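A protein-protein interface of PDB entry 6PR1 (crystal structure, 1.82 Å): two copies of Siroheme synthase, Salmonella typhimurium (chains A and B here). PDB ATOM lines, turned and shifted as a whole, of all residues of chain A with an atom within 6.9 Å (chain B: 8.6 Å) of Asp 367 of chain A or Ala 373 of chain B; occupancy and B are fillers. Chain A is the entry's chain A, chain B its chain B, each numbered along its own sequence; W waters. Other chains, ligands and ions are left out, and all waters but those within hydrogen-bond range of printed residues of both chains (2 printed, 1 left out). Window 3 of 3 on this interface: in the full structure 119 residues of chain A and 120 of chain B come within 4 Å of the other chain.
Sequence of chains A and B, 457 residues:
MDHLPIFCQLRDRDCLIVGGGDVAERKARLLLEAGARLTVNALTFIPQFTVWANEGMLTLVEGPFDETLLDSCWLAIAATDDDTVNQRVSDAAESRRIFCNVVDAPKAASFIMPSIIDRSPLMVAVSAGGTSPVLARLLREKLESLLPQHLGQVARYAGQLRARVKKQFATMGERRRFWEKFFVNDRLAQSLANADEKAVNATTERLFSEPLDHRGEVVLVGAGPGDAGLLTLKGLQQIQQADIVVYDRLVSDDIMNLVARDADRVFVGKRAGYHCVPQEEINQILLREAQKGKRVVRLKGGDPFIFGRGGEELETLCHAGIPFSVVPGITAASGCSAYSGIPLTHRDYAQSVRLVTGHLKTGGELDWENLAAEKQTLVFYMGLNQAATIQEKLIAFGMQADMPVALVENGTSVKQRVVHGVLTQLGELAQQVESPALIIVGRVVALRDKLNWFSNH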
ATOM      1  N   ARG A 354     -10.102 -30.631   7.140  1.00  0.00           N
ATOM      2  CA  ARG A 354     -10.025 -29.296   6.553  1.00  0.00           C
ATOM      3  C   ARG A 354      -9.322 -28.347   7.515  1.00  0.00           C
ATOM      4  O   ARG A 354      -9.808 -28.104   8.625  1.00  0.00           O
ATOM      5  CB  ARG A 354     -11.423 -28.746   6.228  1.00  0.00           C
ATOM      6  CG  ARG A 354     -12.360 -29.732   5.600  1.00  0.00           C
ATOM      7  CD  ARG A 354     -12.231 -29.749   4.099  1.00  0.00           C
ATOM      8  NE  ARG A 354     -12.366 -28.426   3.490  1.00  0.00           N
ATOM      9  CZ  ARG A 354     -13.507 -27.926   3.024  1.00  0.00           C
ATOM     10  NH1 ARG A 354     -14.624 -28.629   3.091  1.00  0.00           N
ATOM     11  NH2 ARG A 354     -13.521 -26.722   2.470  1.00  0.00           N
ATOM     12  N   LEU A 360      -9.698 -13.646   7.002  1.00  0.00           N
ATOM     13  CA  LEU A 360      -9.472 -13.558   5.563  1.00  0.00           C
ATOM     14  C   LEU A 360      -9.237 -12.105   5.137  1.00  0.00           C
ATOM     15  O   LEU A 360      -9.146 -11.190   5.960  1.00  0.00           O
ATOM     16  CB  LEU A 360     -10.663 -14.146   4.805  1.00  0.00           C
ATOM     17  CG  LEU A 360     -10.722 -15.658   4.617  1.00  0.00           C
ATOM     18  CD1 LEU A 360     -11.068 -16.341   5.927  1.00  0.00           C
ATOM     19  CD2 LEU A 360     -11.775 -15.936   3.578  1.00  0.00           C
ATOM     20  N   GLU A 365     -15.035 -14.077   1.890  1.00  0.00           N
ATOM     21  CA  GLU A 365     -15.719 -14.838   2.925  1.00  0.00           C
ATOM     22  C   GLU A 365     -15.635 -16.331   2.614  1.00  0.00           C
ATOM     23  O   GLU A 365     -15.472 -16.747   1.464  1.00  0.00           O
ATOM     24  CB  GLU A 365     -17.184 -14.375   3.087  1.00  0.00           C
ATOM     25  CG  GLU A 365     -18.140 -15.444   3.612  1.00  0.00           C
ATOM     26  CD  GLU A 365     -19.374 -14.880   4.283  1.00  0.00           C
ATOM     27  OE1 GLU A 365     -20.334 -14.521   3.570  1.00  0.00           O
ATOM     28  OE2 GLU A 365     -19.382 -14.808   5.533  1.00  0.00           O
ATOM     29  N   LEU A 366     -15.729 -17.135   3.669  1.00  0.00           N
ATOM     30  CA  LEU A 366     -15.623 -18.580   3.567  1.00  0.00           C
ATOM     31  C   LEU A 366     -16.811 -19.179   2.801  1.00  0.00           C
ATOM     32  O   LEU A 366     -17.895 -18.592   2.708  1.00  0.00           O
ATOM     33  CB  LEU A 366     -15.519 -19.185   4.966  1.00  0.00           C
ATOM     34  CG  LEU A 366     -14.240 -18.829   5.735  1.00  0.00           C
ATOM     35  CD1 LEU A 366     -14.251 -19.449   7.124  1.00  0.00           C
ATOM     36  CD2 LEU A 366     -12.996 -19.287   4.970  1.00  0.00           C
ATOM     37  N   ASP A 367     -16.580 -20.371   2.244  1.00  0.00           N
ATOM     38  CA  ASP A 367     -17.572 -21.111   1.455  1.00  0.00           C
ATOM     39  C   ASP A 367     -18.333 -22.038   2.399  1.00  0.00           C
ATOM     40  O   ASP A 367     -18.037 -23.230   2.536  1.00  0.00           O
ATOM     41  CB  ASP A 367     -16.879 -21.880   0.337  1.00  0.00           C
ATOM     42  CG  ASP A 367     -17.849 -22.558  -0.607  1.00  0.00           C
ATOM     43  OD1 ASP A 367     -19.070 -22.321  -0.501  1.00  0.00           O
ATOM     44  OD2 ASP A 367     -17.380 -23.339  -1.464  1.00  0.00           O
ATOM     45  N   TRP A 368     -19.343 -21.468   3.072  1.00  0.00           N
ATOM     46  CA  TRP A 368     -19.944 -22.170   4.205  1.00  0.00           C
ATOM     47  C   TRP A 368     -20.640 -23.450   3.766  1.00  0.00           C
ATOM     48  O   TRP A 368     -20.618 -24.448   4.497  1.00  0.00           O
ATOM     49  CB  TRP A 368     -20.917 -21.250   4.941  1.00  0.00           C
ATOM     50  CG  TRP A 368     -20.246 -20.051   5.518  1.00  0.00           C
ATOM     51  CD1 TRP A 368     -20.356 -18.761   5.086  1.00  0.00           C
ATOM     52  CD2 TRP A 368     -19.336 -20.031   6.620  1.00  0.00           C
ATOM     53  NE1 TRP A 368     -19.577 -17.939   5.859  1.00  0.00           N
ATOM     54  CE2 TRP A 368     -18.942 -18.690   6.811  1.00  0.00           C
ATOM     55  CE3 TRP A 368     -18.822 -21.016   7.469  1.00  0.00           C
ATOM     56  CZ2 TRP A 368     -18.063 -18.309   7.818  1.00  0.00           C
ATOM     57  CZ3 TRP A 368     -17.943 -20.639   8.467  1.00  0.00           C
ATOM     58  CH2 TRP A 368     -17.571 -19.298   8.630  1.00  0.00           C
ATOM     59  N   GLU A 369     -21.260 -23.443   2.580  1.00  0.00           N
ATOM     60  CA  GLU A 369     -21.879 -24.663   2.063  1.00  0.00           C
ATOM     61  C   GLU A 369     -20.844 -25.776   1.952  1.00  0.00           C
ATOM     62  O   GLU A 369     -21.115 -26.932   2.301  1.00  0.00           O
ATOM     63  CB  GLU A 369     -22.541 -24.391   0.702  1.00  0.00           C
ATOM     64  CG  GLU A 369     -21.557 -24.292  -0.480  1.00  0.00           C
ATOM     65  CD  GLU A 369     -22.203 -23.908  -1.799  1.00  0.00           C
ATOM     66  OE1 GLU A 369     -23.186 -24.568  -2.195  1.00  0.00           O
ATOM     67  OE2 GLU A 369     -21.714 -22.955  -2.446  1.00  0.00           O
ATOM     68  N   ASN A 370     -19.631 -25.425   1.517  1.00  0.00           N
ATOM     69  CA  ASN A 370     -18.541 -26.384   1.404  1.00  0.00           C
ATOM     70  C   ASN A 370     -18.120 -26.895   2.775  1.00  0.00           C
ATOM     71  O   ASN A 370     -17.949 -28.103   2.969  1.00  0.00           O
ATOM     72  CB  ASN A 370     -17.376 -25.714   0.676  1.00  0.00           C
ATOM     73  CG  ASN A 370     -16.432 -26.704   0.029  1.00  0.00           C
ATOM     74  OD1 ASN A 370     -15.402 -27.052   0.603  1.00  0.00           O
ATOM     75  ND2 ASN A 370     -16.762 -27.139  -1.183  1.00  0.00           N
ATOM     76  N   LEU A 371     -17.985 -25.989   3.752  1.00  0.00           N
ATOM     77  CA  LEU A 371     -17.471 -26.382   5.058  1.00  0.00           C
ATOM     78  C   LEU A 371     -18.480 -27.215   5.836  1.00  0.00           C
ATOM     79  O   LEU A 371     -18.088 -28.040   6.670  1.00  0.00           O
ATOM     80  CB  LEU A 371     -17.095 -25.135   5.859  1.00  0.00           C
ATOM     81  CG  LEU A 371     -16.081 -24.233   5.157  1.00  0.00           C
ATOM     82  CD1 LEU A 371     -15.748 -23.033   6.023  1.00  0.00           C
ATOM     83  CD2 LEU A 371     -14.833 -25.032   4.856  1.00  0.00           C
ATOM     84  N   ALA A 372     -19.774 -27.023   5.584  1.00  0.00           N
ATOM     85  CA  ALA A 372     -20.780 -27.683   6.405  1.00  0.00           C
ATOM     86  C   ALA A 372     -21.004 -29.150   6.040  1.00  0.00           C
ATOM     87  O   ALA A 372     -21.773 -29.824   6.736  1.00  0.00           O
ATOM     88  CB  ALA A 372     -22.104 -26.910   6.330  1.00  0.00           C
ATOM     89  N   PHE A 397     -26.157 -23.647   7.031  1.00  0.00           N
ATOM     90  CA  PHE A 397     -25.886 -24.481   5.869  1.00  0.00           C
ATOM     91  C   PHE A 397     -25.951 -25.970   6.199  1.00  0.00           C
ATOM     92  O   PHE A 397     -25.404 -26.795   5.462  1.00  0.00           O
ATOM     93  CB  PHE A 397     -24.546 -24.084   5.240  1.00  0.00           C
ATOM     94  CG  PHE A 397     -24.642 -22.827   4.422  1.00  0.00           C
ATOM     95  CD1 PHE A 397     -24.404 -21.588   4.994  1.00  0.00           C
ATOM     96  CD2 PHE A 397     -25.060 -22.871   3.099  1.00  0.00           C
ATOM     97  CE1 PHE A 397     -24.549 -20.418   4.251  1.00  0.00           C
ATOM     98  CE2 PHE A 397     -25.197 -21.707   2.350  1.00  0.00           C
ATOM     99  CZ  PHE A 397     -24.944 -20.480   2.930  1.00  0.00           C
ATOM    100  N   TYR B 349      -4.361 -17.695  -2.072  1.00  0.00           N
ATOM    101  CA  TYR B 349      -4.555 -18.836  -2.966  1.00  0.00           C
ATOM    102  C   TYR B 349      -5.590 -19.812  -2.418  1.00  0.00           C
ATOM    103  O   TYR B 349      -6.430 -20.329  -3.167  1.00  0.00           O
ATOM    104  CB  TYR B 349      -3.236 -19.576  -3.192  1.00  0.00           C
ATOM    105  CG  TYR B 349      -2.284 -18.916  -4.166  1.00  0.00           C
ATOM    106  CD1 TYR B 349      -2.369 -17.562  -4.448  1.00  0.00           C
ATOM    107  CD2 TYR B 349      -1.313 -19.665  -4.821  1.00  0.00           C
ATOM    108  CE1 TYR B 349      -1.498 -16.963  -5.343  1.00  0.00           C
ATOM    109  CE2 TYR B 349      -0.444 -19.076  -5.729  1.00  0.00           C
ATOM    110  CZ  TYR B 349      -0.530 -17.730  -5.973  1.00  0.00           C
ATOM    111  OH  TYR B 349       0.343 -17.158  -6.876  1.00  0.00           O
ATOM    112  N   GLN B 351      -8.238 -20.706   0.996  1.00  0.00           N
ATOM    113  CA  GLN B 351      -8.840 -20.485   2.304  1.00  0.00           C
ATOM    114  C   GLN B 351      -8.785 -21.729   3.169  1.00  0.00           C
ATOM    115  O   GLN B 351      -8.955 -21.642   4.394  1.00  0.00           O
ATOM    116  CB  GLN B 351     -10.297 -20.034   2.147  1.00  0.00           C
ATOM    117  CG  GLN B 351     -10.487 -18.811   1.267  1.00  0.00           C
ATOM    118  CD  GLN B 351     -11.959 -18.472   1.031  1.00  0.00           C
ATOM    119  OE1 GLN B 351     -12.317 -17.310   0.877  1.00  0.00           O
ATOM    120  NE2 GLN B 351     -12.811 -19.493   1.001  1.00  0.00           N
ATOM    121  N   SER B 352      -8.541 -22.885   2.568  1.00  0.00           N
ATOM    122  CA  SER B 352      -8.467 -24.104   3.350  1.00  0.00           C
ATOM    123  C   SER B 352      -7.593 -25.129   2.647  1.00  0.00           C
ATOM    124  O   SER B 352      -7.445 -25.116   1.420  1.00  0.00           O
ATOM    125  CB  SER B 352      -9.863 -24.672   3.621  1.00  0.00           C
ATOM    126  OG  SER B 352     -10.521 -25.015   2.423  1.00  0.00           O
ATOM    127  N   ARG B 354      -7.234 -29.257   2.360  1.00  0.00           N
ATOM    128  CA  ARG B 354      -8.022 -30.462   2.568  1.00  0.00           C
ATOM    129  C   ARG B 354      -7.118 -31.678   2.470  1.00  0.00           C
ATOM    130  O   ARG B 354      -6.504 -31.919   1.425  1.00  0.00           O
ATOM    131  CB  ARG B 354      -9.164 -30.576   1.572  1.00  0.00           C
ATOM    132  CG  ARG B 354     -10.140 -31.635   2.020  1.00  0.00           C
ATOM    133  CD  ARG B 354     -11.053 -32.008   0.910  1.00  0.00           C
ATOM    134  NE  ARG B 354     -11.859 -30.875   0.498  1.00  0.00           N
ATOM    135  CZ  ARG B 354     -13.175 -30.813   0.624  1.00  0.00           C
ATOM    136  NH1 ARG B 354     -13.848 -31.829   1.157  1.00  0.00           N
ATOM    137  NH2 ARG B 354     -13.809 -29.729   0.210  1.00  0.00           N
ATOM    138  N   ASP B 367     -17.076 -36.667  -2.187  1.00  0.00           N
ATOM    139  CA  ASP B 367     -18.045 -35.621  -2.528  1.00  0.00           C
ATOM    140  C   ASP B 367     -17.399 -34.730  -3.584  1.00  0.00           C
ATOM    141  O   ASP B 367     -16.714 -33.751  -3.274  1.00  0.00           O
ATOM    142  CB  ASP B 367     -18.432 -34.849  -1.273  1.00  0.00           C
ATOM    143  CG  ASP B 367     -19.637 -33.939  -1.466  1.00  0.00           C
ATOM    144  OD1 ASP B 367     -20.200 -33.855  -2.588  1.00  0.00           O
ATOM    145  OD2 ASP B 367     -20.016 -33.288  -0.465  1.00  0.00           O
ATOM    146  N   TRP B 368     -17.616 -35.076  -4.855  1.00  0.00           N
ATOM    147  CA  TRP B 368     -16.812 -34.498  -5.930  1.00  0.00           C
ATOM    148  C   TRP B 368     -17.113 -33.020  -6.139  1.00  0.00           C
ATOM    149  O   TRP B 368     -16.203 -32.229  -6.420  1.00  0.00           O
ATOM    150  CB  TRP B 368     -17.041 -35.277  -7.223  1.00  0.00           C
ATOM    151  CG  TRP B 368     -16.476 -36.645  -7.184  1.00  0.00           C
ATOM    152  CD1 TRP B 368     -17.159 -37.821  -7.289  1.00  0.00           C
ATOM    153  CD2 TRP B 368     -15.102 -36.991  -7.011  1.00  0.00           C
ATOM    154  NE1 TRP B 368     -16.290 -38.878  -7.199  1.00  0.00           N
ATOM    155  CE2 TRP B 368     -15.020 -38.395  -7.028  1.00  0.00           C
ATOM    156  CE3 TRP B 368     -13.929 -36.246  -6.852  1.00  0.00           C
ATOM    157  CZ2 TRP B 368     -13.812 -39.072  -6.892  1.00  0.00           C
ATOM    158  CZ3 TRP B 368     -12.730 -36.917  -6.713  1.00  0.00           C
ATOM    159  CH2 TRP B 368     -12.680 -38.318  -6.734  1.00  0.00           C
ATOM    160  N   GLU B 369     -18.383 -32.628  -6.034  1.00  0.00           N
ATOM    161  CA  GLU B 369     -18.720 -31.210  -6.126  1.00  0.00           C
ATOM    162  C   GLU B 369     -18.035 -30.421  -5.021  1.00  0.00           C
ATOM    163  O   GLU B 369     -17.568 -29.298  -5.241  1.00  0.00           O
ATOM    164  CB  GLU B 369     -20.233 -31.021  -6.057  1.00  0.00           C
ATOM    165  CG  GLU B 369     -20.661 -29.563  -5.995  1.00  0.00           C
ATOM    166  CD  GLU B 369     -22.163 -29.397  -5.979  1.00  0.00           C
ATOM    167  OE1 GLU B 369     -22.870 -30.427  -6.003  1.00  0.00           O
ATOM    168  OE2 GLU B 369     -22.636 -28.240  -5.943  1.00  0.00           O
ATOM    169  N   ASN B 370     -17.968 -31.004  -3.822  1.00  0.00           N
ATOM    170  CA  ASN B 370     -17.286 -30.370  -2.701  1.00  0.00           C
ATOM    171  C   ASN B 370     -15.790 -30.260  -2.960  1.00  0.00           C
ATOM    172  O   ASN B 370     -15.176 -29.227  -2.668  1.00  0.00           O
ATOM    173  CB  ASN B 370     -17.551 -31.169  -1.423  1.00  0.00           C
ATOM    174  CG  ASN B 370     -17.504 -30.314  -0.174  1.00  0.00           C
ATOM    175  OD1 ASN B 370     -16.494 -30.279   0.533  1.00  0.00           O
ATOM    176  ND2 ASN B 370     -18.606 -29.627   0.112  1.00  0.00           N
ATOM    177  N   LEU B 371     -15.182 -31.313  -3.505  1.00  0.00           N
ATOM    178  CA  LEU B 371     -13.743 -31.277  -3.747  1.00  0.00           C
ATOM    179  C   LEU B 371     -13.376 -30.275  -4.839  1.00  0.00           C
ATOM    180  O   LEU B 371     -12.275 -29.710  -4.819  1.00  0.00           O
ATOM    181  CB  LEU B 371     -13.245 -32.675  -4.113  1.00  0.00           C
ATOM    182  CG  LEU B 371     -13.229 -33.655  -2.942  1.00  0.00           C
ATOM    183  CD1 LEU B 371     -13.032 -35.078  -3.425  1.00  0.00           C
ATOM    184  CD2 LEU B 371     -12.117 -33.280  -2.022  1.00  0.00           C
ATOM    185  N   ALA B 372     -14.291 -30.018  -5.774  1.00  0.00           N
ATOM    186  CA  ALA B 372     -13.987 -29.179  -6.927  1.00  0.00           C
ATOM    187  C   ALA B 372     -14.067 -27.681  -6.641  1.00  0.00           C
ATOM    188  O   ALA B 372     -13.686 -26.888  -7.512  1.00  0.00           O
ATOM    189  CB  ALA B 372     -14.929 -29.524  -8.082  1.00  0.00           C
ATOM    190  N   ALA B 373     -14.543 -27.277  -5.465  1.00  0.00           N
ATOM    191  CA  ALA B 373     -14.778 -25.865  -5.182  1.00  0.00           C
ATOM    192  C   ALA B 373     -13.467 -25.083  -5.155  1.00  0.00           C
ATOM    193  O   ALA B 373     -12.400 -25.626  -4.854  1.00  0.00           O
ATOM    194  CB  ALA B 373     -15.514 -25.703  -3.848  1.00  0.00           C
ATOM    195  N   GLU B 374     -13.562 -23.787  -5.462  1.00  0.00           N
ATOM    196  CA  GLU B 374     -12.396 -22.927  -5.608  1.00  0.00           C
ATOM    197  C   GLU B 374     -11.779 -22.595  -4.251  1.00  0.00           C
ATOM    198  O   GLU B 374     -12.373 -22.817  -3.195  1.00  0.00           O
ATOM    199  CB  GLU B 374     -12.768 -21.640  -6.343  1.00  0.00           C
ATOM    200  CG  GLU B 374     -13.220 -21.854  -7.765  1.00  0.00           C
ATOM    201  CD  GLU B 374     -13.573 -20.554  -8.467  1.00  0.00           C
ATOM    202  OE1 GLU B 374     -13.804 -19.541  -7.766  1.00  0.00           O
ATOM    203  OE2 GLU B 374     -13.626 -20.549  -9.717  1.00  0.00           O
ATOM    204  N   LYS B 375     -10.545 -22.077  -4.298  1.00  0.00           N
ATOM    205  CA  LYS B 375      -9.828 -21.574  -3.119  1.00  0.00           C
ATOM    206  C   LYS B 375      -9.495 -22.685  -2.126  1.00  0.00           C
ATOM    207  O   LYS B 375      -9.557 -22.481  -0.912  1.00  0.00           O
ATOM    208  CB  LYS B 375     -10.607 -20.455  -2.413  1.00  0.00           C
ATOM    209  CG  LYS B 375     -10.972 -19.244  -3.275  1.00  0.00           C
ATOM    210  CD  LYS B 375      -9.878 -18.194  -3.258  1.00  0.00           C
ATOM    211  CE  LYS B 375      -9.053 -18.266  -4.525  1.00  0.00           C
ATOM    212  NZ  LYS B 375      -8.393 -16.976  -4.902  1.00  0.00           N
ATOM    213  N   GLN B 376      -9.107 -23.856  -2.632  1.00  0.00           N
ATOM    214  CA  GLN B 376      -8.643 -24.953  -1.790  1.00  0.00           C
ATOM    215  C   GLN B 376      -7.287 -25.445  -2.272  1.00  0.00           C
ATOM    216  O   GLN B 376      -6.952 -25.317  -3.452  1.00  0.00           O
ATOM    217  CB  GLN B 376      -9.590 -26.152  -1.819  1.00  0.00           C
ATOM    218  CG  GLN B 376     -11.024 -25.887  -1.427  1.00  0.00           C
ATOM    219  CD  GLN B 376     -11.849 -27.163  -1.492  1.00  0.00           C
ATOM    220  OE1 GLN B 376     -11.806 -27.994  -0.573  1.00  0.00           O
ATOM    221  NE2 GLN B 376     -12.590 -27.332  -2.573  1.00  0.00           N
ATOM    222  N   THR B 377      -6.532 -26.036  -1.356  1.00  0.00           N
ATOM    223  CA  THR B 377      -5.419 -26.911  -1.695  1.00  0.00           C
ATOM    224  C   THR B 377      -5.837 -28.332  -1.333  1.00  0.00           C
ATOM    225  O   THR B 377      -6.052 -28.635  -0.152  1.00  0.00           O
ATOM    226  CB  THR B 377      -4.141 -26.519  -0.949  1.00  0.00           C
ATOM    227  OG1 THR B 377      -3.768 -25.168  -1.282  1.00  0.00           O
ATOM    228  CG2 THR B 377      -3.009 -27.484  -1.320  1.00  0.00           C
ATOM    229  N   LEU B 378      -5.962 -29.195  -2.339  1.00  0.00           N
ATOM    230  CA  LEU B 378      -6.338 -30.587  -2.098  1.00  0.00           C
ATOM    231  C   LEU B 378      -5.096 -31.446  -1.951  1.00  0.00           C
ATOM    232  O   LEU B 378      -4.155 -31.328  -2.741  1.00  0.00           O
ATOM    233  CB  LEU B 378      -7.185 -31.135  -3.242  1.00  0.00           C
ATOM    234  CG  LEU B 378      -8.435 -30.356  -3.626  1.00  0.00           C
ATOM    235  CD1 LEU B 378      -9.079 -31.070  -4.813  1.00  0.00           C
ATOM    236  CD2 LEU B 378      -9.390 -30.282  -2.438  1.00  0.00           C
ATOM    237  N   LEU B 394     -13.053 -34.099 -11.040  1.00  0.00           N
ATOM    238  CA  LEU B 394     -12.780 -32.681 -10.815  1.00  0.00           C
ATOM    239  C   LEU B 394     -13.076 -31.861 -12.068  1.00  0.00           C
ATOM    240  O   LEU B 394     -13.660 -30.774 -11.984  1.00  0.00           O
ATOM    241  CB  LEU B 394     -11.332 -32.486 -10.358  1.00  0.00           C
ATOM    242  CG  LEU B 394     -10.976 -32.951  -8.940  1.00  0.00           C
ATOM    243  CD1 LEU B 394      -9.490 -32.722  -8.652  1.00  0.00           C
ATOM    244  CD2 LEU B 394     -11.847 -32.271  -7.874  1.00  0.00           C
ATOM    245  N   PHE B 397     -16.866 -31.551 -12.553  1.00  0.00           N
ATOM    246  CA  PHE B 397     -17.554 -30.738 -11.561  1.00  0.00           C
ATOM    247  C   PHE B 397     -17.031 -29.309 -11.510  1.00  0.00           C
ATOM    248  O   PHE B 397     -17.193 -28.629 -10.490  1.00  0.00           O
ATOM    249  CB  PHE B 397     -17.476 -31.401 -10.184  1.00  0.00           C
ATOM    250  CG  PHE B 397     -18.451 -32.534 -10.012  1.00  0.00           C
ATOM    251  CD1 PHE B 397     -18.060 -33.843 -10.233  1.00  0.00           C
ATOM    252  CD2 PHE B 397     -19.769 -32.284  -9.661  1.00  0.00           C
ATOM    253  CE1 PHE B 397     -18.953 -34.884 -10.087  1.00  0.00           C
ATOM    254  CE2 PHE B 397     -20.668 -33.321  -9.513  1.00  0.00           C
ATOM    255  CZ  PHE B 397     -20.257 -34.624  -9.726  1.00  0.00           C
ATOM    256  N   GLY B 398     -16.397 -28.847 -12.584  1.00  0.00           N
ATOM    257  CA  GLY B 398     -16.150 -27.435 -12.779  1.00  0.00           C
ATOM    258  C   GLY B 398     -14.797 -26.905 -12.363  1.00  0.00           C
ATOM    259  O   GLY B 398     -14.606 -25.683 -12.391  1.00  0.00           O
ATOM    260  N   MET B 399     -13.860 -27.761 -11.962  1.00  0.00           N
ATOM    261  CA  MET B 399     -12.519 -27.271 -11.671  1.00  0.00           C
ATOM    262  C   MET B 399     -11.819 -26.910 -12.974  1.00  0.00           C
ATOM    263  O   MET B 399     -11.841 -27.684 -13.935  1.00  0.00           O
ATOM    264  CB  MET B 399     -11.696 -28.307 -10.907  1.00  0.00           C
ATOM    265  CG  MET B 399     -10.250 -27.858 -10.712  1.00  0.00           C
ATOM    266  SD  MET B 399      -9.221 -28.882  -9.643  1.00  0.00           S
ATOM    267  CE  MET B 399      -9.841 -28.429  -8.022  1.00  0.00           C
ATOM    268  N   GLN B 400     -11.201 -25.732 -13.004  1.00  0.00           N
ATOM    269  CA  GLN B 400     -10.552 -25.243 -14.213  1.00  0.00           C
ATOM    270  C   GLN B 400      -9.491 -26.223 -14.699  1.00  0.00           C
ATOM    271  O   GLN B 400      -8.684 -26.727 -13.912  1.00  0.00           O
ATOM    272  CB  GLN B 400      -9.934 -23.873 -13.948  1.00  0.00           C
ATOM    273  CG  GLN B 400     -10.950 -22.843 -13.479  1.00  0.00           C
ATOM    274  CD  GLN B 400     -10.510 -21.418 -13.748  1.00  0.00           C
ATOM    275  OE1 GLN B 400      -9.320 -21.142 -13.916  1.00  0.00           O
ATOM    276  NE2 GLN B 400     -11.473 -20.505 -13.804  1.00  0.00           N
ATOM    277  N   MET B 403      -5.723 -25.953 -13.743  1.00  0.00           N
ATOM    278  CA  MET B 403      -5.315 -25.989 -12.344  1.00  0.00           C
ATOM    279  C   MET B 403      -4.031 -26.800 -12.201  1.00  0.00           C
ATOM    280  O   MET B 403      -3.981 -27.949 -12.645  1.00  0.00           O
ATOM    281  CB  MET B 403      -6.417 -26.594 -11.481  1.00  0.00           C
ATOM    282  CG  MET B 403      -6.065 -26.648 -10.000  1.00  0.00           C
ATOM    283  SD  MET B 403      -6.050 -24.991  -9.292  1.00  0.00           S
ATOM    284  CE  MET B 403      -7.770 -24.508  -9.475  1.00  0.00           C
ATOM    285  N   VAL B 441      -3.359 -30.740  -5.494  1.00  0.00           N
ATOM    286  CA  VAL B 441      -4.134 -30.013  -6.490  1.00  0.00           C
ATOM    287  C   VAL B 441      -4.417 -28.615  -5.951  1.00  0.00           C
ATOM    288  O   VAL B 441      -5.021 -28.474  -4.883  1.00  0.00           O
ATOM    289  CB  VAL B 441      -5.455 -30.734  -6.803  1.00  0.00           C
ATOM    290  CG1 VAL B 441      -6.250 -29.967  -7.860  1.00  0.00           C
ATOM    291  CG2 VAL B 441      -5.192 -32.165  -7.243  1.00  0.00           C
ATOM    292  N   GLY B 442      -4.014 -27.591  -6.688  1.00  0.00           N
ATOM    293  CA  GLY B 442      -4.339 -26.226  -6.310  1.00  0.00           C
ATOM    294  C   GLY B 442      -3.329 -25.236  -6.855  1.00  0.00           C
ATOM    295  O   GLY B 442      -2.236 -25.590  -7.293  1.00  0.00           O
HETATM  296  O   HOH W   1     -10.289 -27.415   1.775  1.00  0.00           O
HETATM  297  O   HOH W   2     -13.921 -21.427   2.214  1.00  0.00           O
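Arg 354 of chain A touches its own counterpart, Arg 354 of chain B.
Arg 354 of chain A touches Asn 370 of chain B, and with the chains exchanged Asn 370 of chain A touches Arg 354 of chain B.
Of the 12 pairs that touch across the chains among the printed residues, 4 have their exchanged pair printed and touching as well.
Among the printed residues, merely in contact across the chains: Leu 360 of chain A with Gln 351 of chain B, Asn 370 of chain A with Ala 373 of chain B, Arg 354 of chain A with Asn 370 of chain B, Arg 354 of chain A with Gln 376 of chain B, Asp 367 of chain A with Ala 373 of chain B, Asn 370 of chain A with Gln 376 of chain B and Leu 366 of chain A with Gln 351 of chain B.
The guanidinium group (NH2) of Arg 354 of chain A is in hydrogen-bond range of the side-chain amide oxygen (OD1) of Asn 370 of chain A (2.7 Å).
The side-chain amide oxygen (OE1) of Gln 376 of chain B is in hydrogen-bond range of the guanidinium group (NH2) of Arg 354 of chain B, 2.8 Å away.
Water W1 lies within hydrogen-bond range of OG of Ser 352 of chain B, OE1 of Gln 376 of chain B and NE of Arg 354 of chain A.
Water W2 lies within hydrogen-bond range of NE2 of Gln 351 of chain B (2.5 Å) and N of Asp 367 of chain A (2.9 Å).
The guanidinium group (NH2) of Arg 354 of chain A sits at hydrogen-bond distance from the side-chain hydroxyl (OG) of Ser 352 of chain B, 3.5 Å away.
The side-chain amide oxygen of Gln 351 of chain B sits close to the backbone carbonyl oxygen of Glu 365 of chain A (3.3 Å).
The side-chain amide oxygen (OD1) of Asn 370 of chain A sits at hydrogen-bond distance from the guanidinium group (NH2) of Arg 354 of chain B, 3.1 Å away.
The backbone carbonyl oxygen of Asn 370 of chain B lies within hydrogen-bond range of the side-chain amide nitrogen of Asn 370 of chain A (3.0 Å).
The guanidinium group of Arg 354 of chain A sits close to the guanidinium group of Arg 354 of chain B, 3.2 Å away.
Asp 367 of chain A touches just one residue of chain B: Ala 373 (3.8 Å).
Of chain A, only Asp 367 and Asn 370 come within 4 Å of Ala 373 of chain B.
Of the printed residues of chain A, Arg 354 of chain B touches Arg 354 and Asn 370.
Of the printed residues of chain B, Leu 366 of chain A touches Gln 351.
Phe 397 of chain B touches none of the printed residues of chain A.
Met 399 of chain B touches none of the printed residues of chain A.
The nearest residue of chain A that does not touch Ala 373 of chain B is Arg 354 of chain A (6.7 Å).
The nearest printed residue of chain B that does not touch Arg 354 of chain A is Ala 373 of chain B (6.7 Å).
Of the 11 printed residues of chain A, 6 touch a printed residue of chain B.
Printed residues of chain A that touch a printed residue of chain B: Arg 354, Leu 360, Glu 365, Leu 366, Asp 367 and Asn 370.
Hydrophobic or aromatic side chains of chain A within 4 Å of the printed part of chain B: Leu 360 and Leu 366.
Hydrophobic or aromatic side chains of chain B that line the printed part of chain A: Ala 373.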
